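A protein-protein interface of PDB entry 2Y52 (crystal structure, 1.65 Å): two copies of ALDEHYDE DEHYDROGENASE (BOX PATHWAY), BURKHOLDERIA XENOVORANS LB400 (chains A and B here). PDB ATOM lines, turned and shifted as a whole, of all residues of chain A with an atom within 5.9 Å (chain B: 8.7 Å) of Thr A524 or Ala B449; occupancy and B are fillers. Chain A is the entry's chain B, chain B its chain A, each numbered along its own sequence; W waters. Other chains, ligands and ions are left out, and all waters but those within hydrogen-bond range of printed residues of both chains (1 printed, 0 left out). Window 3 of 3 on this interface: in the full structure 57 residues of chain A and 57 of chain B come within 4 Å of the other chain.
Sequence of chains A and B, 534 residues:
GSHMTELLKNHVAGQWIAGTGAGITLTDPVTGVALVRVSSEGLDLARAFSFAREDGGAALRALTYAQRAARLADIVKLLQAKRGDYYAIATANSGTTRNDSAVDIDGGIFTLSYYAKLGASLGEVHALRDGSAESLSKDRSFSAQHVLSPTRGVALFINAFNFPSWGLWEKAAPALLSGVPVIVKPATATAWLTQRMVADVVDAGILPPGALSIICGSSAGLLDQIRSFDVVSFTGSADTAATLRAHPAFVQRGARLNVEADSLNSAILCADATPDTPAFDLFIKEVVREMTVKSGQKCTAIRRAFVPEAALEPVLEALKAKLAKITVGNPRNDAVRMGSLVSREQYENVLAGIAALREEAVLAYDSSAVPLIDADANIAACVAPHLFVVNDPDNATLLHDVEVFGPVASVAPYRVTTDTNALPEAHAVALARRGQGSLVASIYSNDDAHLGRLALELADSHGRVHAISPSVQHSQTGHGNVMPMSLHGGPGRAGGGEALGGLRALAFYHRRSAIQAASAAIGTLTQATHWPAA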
ATOM      1  N   SER A 519      -4.142  31.232 -16.021  1.00  0.00           N
ATOM      2  CA  SER A 519      -3.499  32.340 -16.713  1.00  0.00           C
ATOM      3  C   SER A 519      -1.981  32.323 -16.512  1.00  0.00           C
ATOM      4  O   SER A 519      -1.237  32.722 -17.395  1.00  0.00           O
ATOM      5  CB  SER A 519      -4.044  33.739 -16.235  1.00  0.00           C
ATOM      6  OG  SER A 519      -5.483  33.840 -16.394  1.00  0.00           O
ATOM      7  N   ALA A 520      -1.512  31.948 -15.310  1.00  0.00           N
ATOM      8  CA  ALA A 520      -0.043  31.809 -15.128  1.00  0.00           C
ATOM      9  C   ALA A 520       0.582  30.736 -16.042  1.00  0.00           C
ATOM     10  O   ALA A 520       1.715  30.878 -16.455  1.00  0.00           O
ATOM     11  CB  ALA A 520       0.292  31.551 -13.631  1.00  0.00           C
ATOM     12  N   ALA A 521      -0.132  29.666 -16.347  1.00  0.00           N
ATOM     13  CA  ALA A 521       0.423  28.708 -17.305  1.00  0.00           C
ATOM     14  C   ALA A 521       0.454  29.321 -18.726  1.00  0.00           C
ATOM     15  O   ALA A 521       1.375  29.068 -19.469  1.00  0.00           O
ATOM     16  CB  ALA A 521      -0.345  27.365 -17.367  1.00  0.00           C
ATOM     17  N   ILE A 522      -0.576  30.065 -19.117  1.00  0.00           N
ATOM     18  CA  ILE A 522      -0.604  30.690 -20.421  1.00  0.00           C
ATOM     19  C   ILE A 522       0.545  31.753 -20.442  1.00  0.00           C
ATOM     20  O   ILE A 522       1.240  31.915 -21.432  1.00  0.00           O
ATOM     21  CB  ILE A 522      -1.979  31.414 -20.694  1.00  0.00           C
ATOM     22  CG1 ILE A 522      -3.140  30.399 -20.787  1.00  0.00           C
ATOM     23  CG2 ILE A 522      -1.883  32.246 -21.971  1.00  0.00           C
ATOM     24  CD1 ILE A 522      -2.942  29.311 -21.933  1.00  0.00           C
ATOM     25  N   GLY A 523       0.734  32.470 -19.330  1.00  0.00           N
ATOM     26  CA  GLY A 523       1.893  33.393 -19.284  1.00  0.00           C
ATOM     27  C   GLY A 523       3.211  32.643 -19.501  1.00  0.00           C
ATOM     28  O   GLY A 523       4.078  33.106 -20.320  1.00  0.00           O
ATOM     29  N   THR A 524       3.419  31.506 -18.823  1.00  0.00           N
ATOM     30  CA  THR A 524       4.713  30.827 -19.034  1.00  0.00           C
ATOM     31  C   THR A 524       4.859  30.296 -20.445  1.00  0.00           C
ATOM     32  O   THR A 524       5.939  30.473 -20.971  1.00  0.00           O
ATOM     33  CB  THR A 524       5.249  29.852 -17.940  1.00  0.00           C
ATOM     34  OG1 THR A 524       5.498  28.533 -18.443  1.00  0.00           O
ATOM     35  CG2 THR A 524       4.551  29.928 -16.668  1.00  0.00           C
ATOM     36  N   LEU A 525       3.782  29.712 -21.043  1.00  0.00           N
ATOM     37  CA  LEU A 525       3.752  29.252 -22.465  1.00  0.00           C
ATOM     38  C   LEU A 525       4.184  30.414 -23.362  1.00  0.00           C
ATOM     39  O   LEU A 525       5.003  30.249 -24.289  1.00  0.00           O
ATOM     40  CB  LEU A 525       2.278  28.798 -22.972  1.00  0.00           C
ATOM     41  CG  LEU A 525       1.165  27.745 -22.648  1.00  0.00           C
ATOM     42  CD1 LEU A 525      -0.201  28.253 -23.017  1.00  0.00           C
ATOM     43  CD2 LEU A 525       1.442  26.451 -23.406  1.00  0.00           C
ATOM     44  N   THR A 526       3.603  31.582 -23.114  1.00  0.00           N
ATOM     45  CA  THR A 526       3.785  32.709 -23.995  1.00  0.00           C
ATOM     46  C   THR A 526       5.260  33.168 -23.995  1.00  0.00           C
ATOM     47  O   THR A 526       5.784  33.578 -24.988  1.00  0.00           O
ATOM     48  CB  THR A 526       2.868  33.935 -23.696  1.00  0.00           C
ATOM     49  OG1 THR A 526       3.257  34.555 -22.490  1.00  0.00           O
ATOM     50  CG2 THR A 526       1.442  33.557 -23.680  1.00  0.00           C
ATOM     51  N   GLN A 527       5.908  33.049 -22.861  1.00  0.00           N
ATOM     52  CA  GLN A 527       7.334  33.399 -22.768  1.00  0.00           C
ATOM     53  C   GLN A 527       8.242  32.543 -23.637  1.00  0.00           C
ATOM     54  O   GLN A 527       9.402  32.958 -23.914  1.00  0.00           O
ATOM     55  CB  GLN A 527       7.801  33.235 -21.320  1.00  0.00           C
ATOM     56  CG  GLN A 527       7.262  34.349 -20.460  1.00  0.00           C
ATOM     57  CD  GLN A 527       7.785  34.261 -19.070  1.00  0.00           C
ATOM     58  OE1 GLN A 527       8.417  33.282 -18.674  1.00  0.00           O
ATOM     59  NE2 GLN A 527       7.582  35.331 -18.319  1.00  0.00           N
ATOM     60  N   ALA A 528       7.768  31.332 -24.002  1.00  0.00           N
ATOM     61  CA  ALA A 528       8.530  30.350 -24.824  1.00  0.00           C
ATOM     62  C   ALA A 528       8.161  30.400 -26.309  1.00  0.00           C
ATOM     63  O   ALA A 528       8.592  29.496 -27.110  1.00  0.00           O
ATOM     64  CB  ALA A 528       8.293  28.938 -24.297  1.00  0.00           C
ATOM     65  N   LEU B 423      11.068  16.546 -18.636  1.00  0.00           N
ATOM     66  CA  LEU B 423      10.007  16.869 -17.672  1.00  0.00           C
ATOM     67  C   LEU B 423       9.740  15.605 -16.903  1.00  0.00           C
ATOM     68  O   LEU B 423       9.981  14.530 -17.449  1.00  0.00           O
ATOM     69  CB  LEU B 423       8.722  17.308 -18.426  1.00  0.00           C
ATOM     70  CG  LEU B 423       8.794  18.669 -19.115  1.00  0.00           C
ATOM     71  CD1 LEU B 423       7.420  19.078 -19.562  1.00  0.00           C
ATOM     72  CD2 LEU B 423       9.489  19.860 -18.355  1.00  0.00           C
ATOM     73  N   ILE B 443      -4.135  17.750 -18.674  1.00  0.00           N
ATOM     74  CA  ILE B 443      -2.983  17.567 -17.744  1.00  0.00           C
ATOM     75  C   ILE B 443      -3.290  18.214 -16.403  1.00  0.00           C
ATOM     76  O   ILE B 443      -3.909  19.304 -16.349  1.00  0.00           O
ATOM     77  CB  ILE B 443      -1.657  18.180 -18.378  1.00  0.00           C
ATOM     78  CG1 ILE B 443      -1.924  19.552 -19.059  1.00  0.00           C
ATOM     79  CG2 ILE B 443      -1.023  17.225 -19.381  1.00  0.00           C
ATOM     80  CD1 ILE B 443      -0.656  20.314 -19.497  1.00  0.00           C
ATOM     81  N   SER B 445      -1.924  19.306 -12.428  1.00  0.00           N
ATOM     82  CA  SER B 445      -0.804  19.639 -11.565  1.00  0.00           C
ATOM     83  C   SER B 445      -1.225  20.734 -10.549  1.00  0.00           C
ATOM     84  O   SER B 445      -2.188  21.469 -10.772  1.00  0.00           O
ATOM     85  CB  SER B 445       0.360  20.178 -12.445  1.00  0.00           C
ATOM     86  OG  SER B 445       1.560  20.419 -11.654  1.00  0.00           O
ATOM     87  N   ASN B 446      -0.470  20.780  -9.421  1.00  0.00           N
ATOM     88  CA  ASN B 446      -0.532  21.930  -8.483  1.00  0.00           C
ATOM     89  C   ASN B 446       0.262  23.116  -8.970  1.00  0.00           C
ATOM     90  O   ASN B 446       0.014  24.231  -8.512  1.00  0.00           O
ATOM     91  CB  ASN B 446      -0.012  21.526  -7.092  1.00  0.00           C
ATOM     92  CG  ASN B 446      -0.788  20.332  -6.510  1.00  0.00           C
ATOM     93  OD1 ASN B 446      -1.971  20.456  -6.112  1.00  0.00           O
ATOM     94  ND2 ASN B 446      -0.141  19.142  -6.568  1.00  0.00           N
ATOM     95  N   ASP B 447       1.158  22.886  -9.946  1.00  0.00           N
ATOM     96  CA  ASP B 447       2.106  23.947 -10.394  1.00  0.00           C
ATOM     97  C   ASP B 447       1.689  24.542 -11.742  1.00  0.00           C
ATOM     98  O   ASP B 447       2.003  23.937 -12.772  1.00  0.00           O
ATOM     99  CB  ASP B 447       3.546  23.319 -10.482  1.00  0.00           C
ATOM    100  CG  ASP B 447       4.694  24.353 -10.809  1.00  0.00           C
ATOM    101  OD1 ASP B 447       4.527  25.343 -11.511  1.00  0.00           O
ATOM    102  OD2 ASP B 447       5.832  24.083 -10.436  1.00  0.00           O
ATOM    103  N   ASP B 448       1.118  25.743 -11.756  1.00  0.00           N
ATOM    104  CA  ASP B 448       0.623  26.358 -13.042  1.00  0.00           C
ATOM    105  C   ASP B 448       1.740  26.564 -14.090  1.00  0.00           C
ATOM    106  O   ASP B 448       1.576  26.248 -15.291  1.00  0.00           O
ATOM    107  CB  ASP B 448      -0.078  27.720 -12.781  1.00  0.00           C
ATOM    108  CG  ASP B 448      -1.434  27.581 -12.125  1.00  0.00           C
ATOM    109  OD1 ASP B 448      -1.939  26.437 -12.017  1.00  0.00           O
ATOM    110  OD2 ASP B 448      -2.010  28.601 -11.721  1.00  0.00           O
ATOM    111  N   ALA B 449       2.868  27.149 -13.691  1.00  0.00           N
ATOM    112  CA  ALA B 449       4.037  27.288 -14.625  1.00  0.00           C
ATOM    113  C   ALA B 449       4.451  25.968 -15.295  1.00  0.00           C
ATOM    114  O   ALA B 449       4.649  25.916 -16.535  1.00  0.00           O
ATOM    115  CB  ALA B 449       5.268  27.984 -13.900  1.00  0.00           C
ATOM    116  N   HIS B 450       4.484  24.900 -14.502  1.00  0.00           N
ATOM    117  CA  HIS B 450       4.792  23.569 -14.982  1.00  0.00           C
ATOM    118  C   HIS B 450       3.804  23.153 -16.076  1.00  0.00           C
ATOM    119  O   HIS B 450       4.224  22.568 -17.096  1.00  0.00           O
ATOM    120  CB  HIS B 450       4.866  22.550 -13.853  1.00  0.00           C
ATOM    121  CG  HIS B 450       5.406  21.242 -14.298  1.00  0.00           C
ATOM    122  ND1 HIS B 450       6.733  21.057 -14.608  1.00  0.00           N
ATOM    123  CD2 HIS B 450       4.783  20.076 -14.589  1.00  0.00           C
ATOM    124  CE1 HIS B 450       6.913  19.812 -15.037  1.00  0.00           C
ATOM    125  NE2 HIS B 450       5.742  19.205 -15.042  1.00  0.00           N
ATOM    126  N   LEU B 451       2.529  23.479 -15.888  1.00  0.00           N
ATOM    127  CA  LEU B 451       1.524  23.082 -16.897  1.00  0.00           C
ATOM    128  C   LEU B 451       1.755  23.782 -18.257  1.00  0.00           C
ATOM    129  O   LEU B 451       1.603  23.130 -19.300  1.00  0.00           O
ATOM    130  CB  LEU B 451       0.083  23.220 -16.350  1.00  0.00           C
ATOM    131  CG  LEU B 451      -0.315  22.327 -15.152  1.00  0.00           C
ATOM    132  CD1 LEU B 451      -1.633  22.700 -14.581  1.00  0.00           C
ATOM    133  CD2 LEU B 451      -0.426  20.850 -15.737  1.00  0.00           C
ATOM    134  N   GLY B 452       2.112  25.088 -18.239  1.00  0.00           N
ATOM    135  CA  GLY B 452       2.546  25.816 -19.444  1.00  0.00           C
ATOM    136  C   GLY B 452       3.608  25.041 -20.225  1.00  0.00           C
ATOM    137  O   GLY B 452       3.548  24.931 -21.438  1.00  0.00           O
ATOM    138  N   ARG B 453       4.635  24.563 -19.536  1.00  0.00           N
ATOM    139  CA  ARG B 453       5.794  23.945 -20.206  1.00  0.00           C
ATOM    140  C   ARG B 453       5.381  22.595 -20.739  1.00  0.00           C
ATOM    141  O   ARG B 453       5.753  22.240 -21.849  1.00  0.00           O
ATOM    142  CB  ARG B 453       6.992  23.817 -19.224  1.00  0.00           C
ATOM    143  CG  ARG B 453       7.400  25.187 -18.581  1.00  0.00           C
ATOM    144  CD  ARG B 453       8.928  25.344 -18.161  1.00  0.00           C
ATOM    145  NE  ARG B 453       9.179  26.682 -17.560  1.00  0.00           N
ATOM    146  CZ  ARG B 453       8.807  27.021 -16.312  1.00  0.00           C
ATOM    147  NH1 ARG B 453       8.178  26.119 -15.539  1.00  0.00           N
ATOM    148  NH2 ARG B 453       9.050  28.254 -15.828  1.00  0.00           N
ATOM    149  N   LEU B 454       4.611  21.845 -19.945  1.00  0.00           N
ATOM    150  CA  LEU B 454       4.182  20.512 -20.371  1.00  0.00           C
ATOM    151  C   LEU B 454       3.248  20.601 -21.601  1.00  0.00           C
ATOM    152  O   LEU B 454       3.247  19.678 -22.487  1.00  0.00           O
ATOM    153  CB  LEU B 454       3.491  19.793 -19.223  1.00  0.00           C
ATOM    154  CG  LEU B 454       2.903  18.393 -19.439  1.00  0.00           C
ATOM    155  CD1 LEU B 454       3.913  17.425 -20.067  1.00  0.00           C
ATOM    156  CD2 LEU B 454       2.471  17.980 -17.963  1.00  0.00           C
ATOM    157  N   ALA B 455       2.351  21.558 -21.566  1.00  0.00           N
ATOM    158  CA  ALA B 455       1.365  21.750 -22.661  1.00  0.00           C
ATOM    159  C   ALA B 455       2.099  21.801 -23.984  1.00  0.00           C
ATOM    160  O   ALA B 455       1.627  21.246 -24.991  1.00  0.00           O
ATOM    161  CB  ALA B 455       0.480  23.073 -22.408  1.00  0.00           C
ATOM    162  N   LEU B 456       3.199  22.548 -24.085  1.00  0.00           N
ATOM    163  CA  LEU B 456       3.912  22.641 -25.375  1.00  0.00           C
ATOM    164  C   LEU B 456       4.464  21.316 -25.863  1.00  0.00           C
ATOM    165  O   LEU B 456       4.624  21.118 -27.075  1.00  0.00           O
ATOM    166  CB  LEU B 456       5.007  23.725 -25.316  1.00  0.00           C
ATOM    167  CG  LEU B 456       4.501  25.158 -25.138  1.00  0.00           C
ATOM    168  CD1 LEU B 456       5.723  25.995 -24.682  1.00  0.00           C
ATOM    169  CD2 LEU B 456       3.823  25.881 -26.367  1.00  0.00           C
ATOM    170  N   SER B 469      -5.807  22.773 -12.690  1.00  0.00           N
ATOM    171  CA  SER B 469      -5.043  22.920 -11.467  1.00  0.00           C
ATOM    172  C   SER B 469      -5.939  23.681 -10.452  1.00  0.00           C
ATOM    173  O   SER B 469      -6.961  24.297 -10.794  1.00  0.00           O
ATOM    174  CB  SER B 469      -3.738  23.733 -11.739  1.00  0.00           C
ATOM    175  OG  SER B 469      -4.087  24.930 -12.427  1.00  0.00           O
ATOM    176  N   SER B 471      -5.805  26.458  -8.968  1.00  0.00           N
ATOM    177  CA  SER B 471      -6.157  27.869  -9.189  1.00  0.00           C
ATOM    178  C   SER B 471      -7.352  28.072 -10.164  1.00  0.00           C
ATOM    179  O   SER B 471      -7.954  29.155 -10.230  1.00  0.00           O
ATOM    180  CB  SER B 471      -4.916  28.630  -9.676  1.00  0.00           C
ATOM    181  OG  SER B 471      -4.758  28.447 -11.066  1.00  0.00           O
HETATM  182  O   HOH W   1      -2.718  31.377 -12.828  1.00  0.00           O
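The side-chain carboxylate (OD1) of Asp B448 is in hydrogen-bond range of the side-chain hydroxyl (OG) of Ser B469 (2.7 Å). The side-chain carboxylate (OD1) of Asp B447 is in hydrogen-bond range of the backbone NH (N) of Ala B449 (3.3 Å). The side-chain carboxylate of Asp B448 lies within hydrogen-bond range of the side-chain hydroxyl of Ser B471.
Of chain B, only Ala B449 (3.3 Å) and Arg B453 (3.9 Å) come within 4 Å of Thr A524. Of chain A, only Thr A524 comes within 4 Å of Ala B449. No residue of chain B comes within 4 Å of Gly A523. Printed residues of chain A within 4 Å of Arg B453: Thr A524. Of the printed residues of chain A, Asp B448 touches Ala A520 (3.9 Å) and Ala A521 (3.0 Å). Of the printed residues of chain A, Gly B452 touches Ala A521 (3.5 Å) and Leu A525 (3.3 Å). Gln A527 touches none of the printed residues of chain B. The nearest residue of chain B that does not touch Thr A524 is Gly B452 (4.1 Å).
Of the 16 printed residues of chain B, 6 touch a printed residue of chain A. Printed residues of chain A that touch a printed residue of chain B: Ala A520, Ala A521, Thr A524, Leu A525 and Ala A528. Hydrophobic or aromatic side chains of chain A within 4 Å of the printed part of chain B: Ala A520, Ala A521, Leu A525 and Ala A528. Along chain A the printed residues that touch a printed residue of chain B span positions 520 to 528.
O of Ala B449 sits at hydrogen-bond distance from OG1 of Thr A524.
No position is printed for both chains. Of the 9 pairs that touch across the chains among the printed residues, none has its exchanged pair printed and touching as well.
Water W1 lies within hydrogen-bond range of the backbone NH (N) of Ala A520, the side-chain carboxylate (OD2) of Asp B448 and the backbone NH (N) of Ser A519.
Ala A520 touches Asp B448 (CB to CB, 3.9 Å). Ala A521 touches Asp B448 (CB to O, 3.0 Å). Ala A521 touches Gly B452. CG of Arg B453 touches OG1 of Thr A524, at 3.9 Å. CD2 of Leu A525 touches O of Gly B452, at 3.3 Å. CD2 of Leu A525 touches CB of Ala B455, 3.7 Å away. Leu A525 touches Leu B456. Leu B456 touches Ala A528 (CD1 to CB, 3.9 Å).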
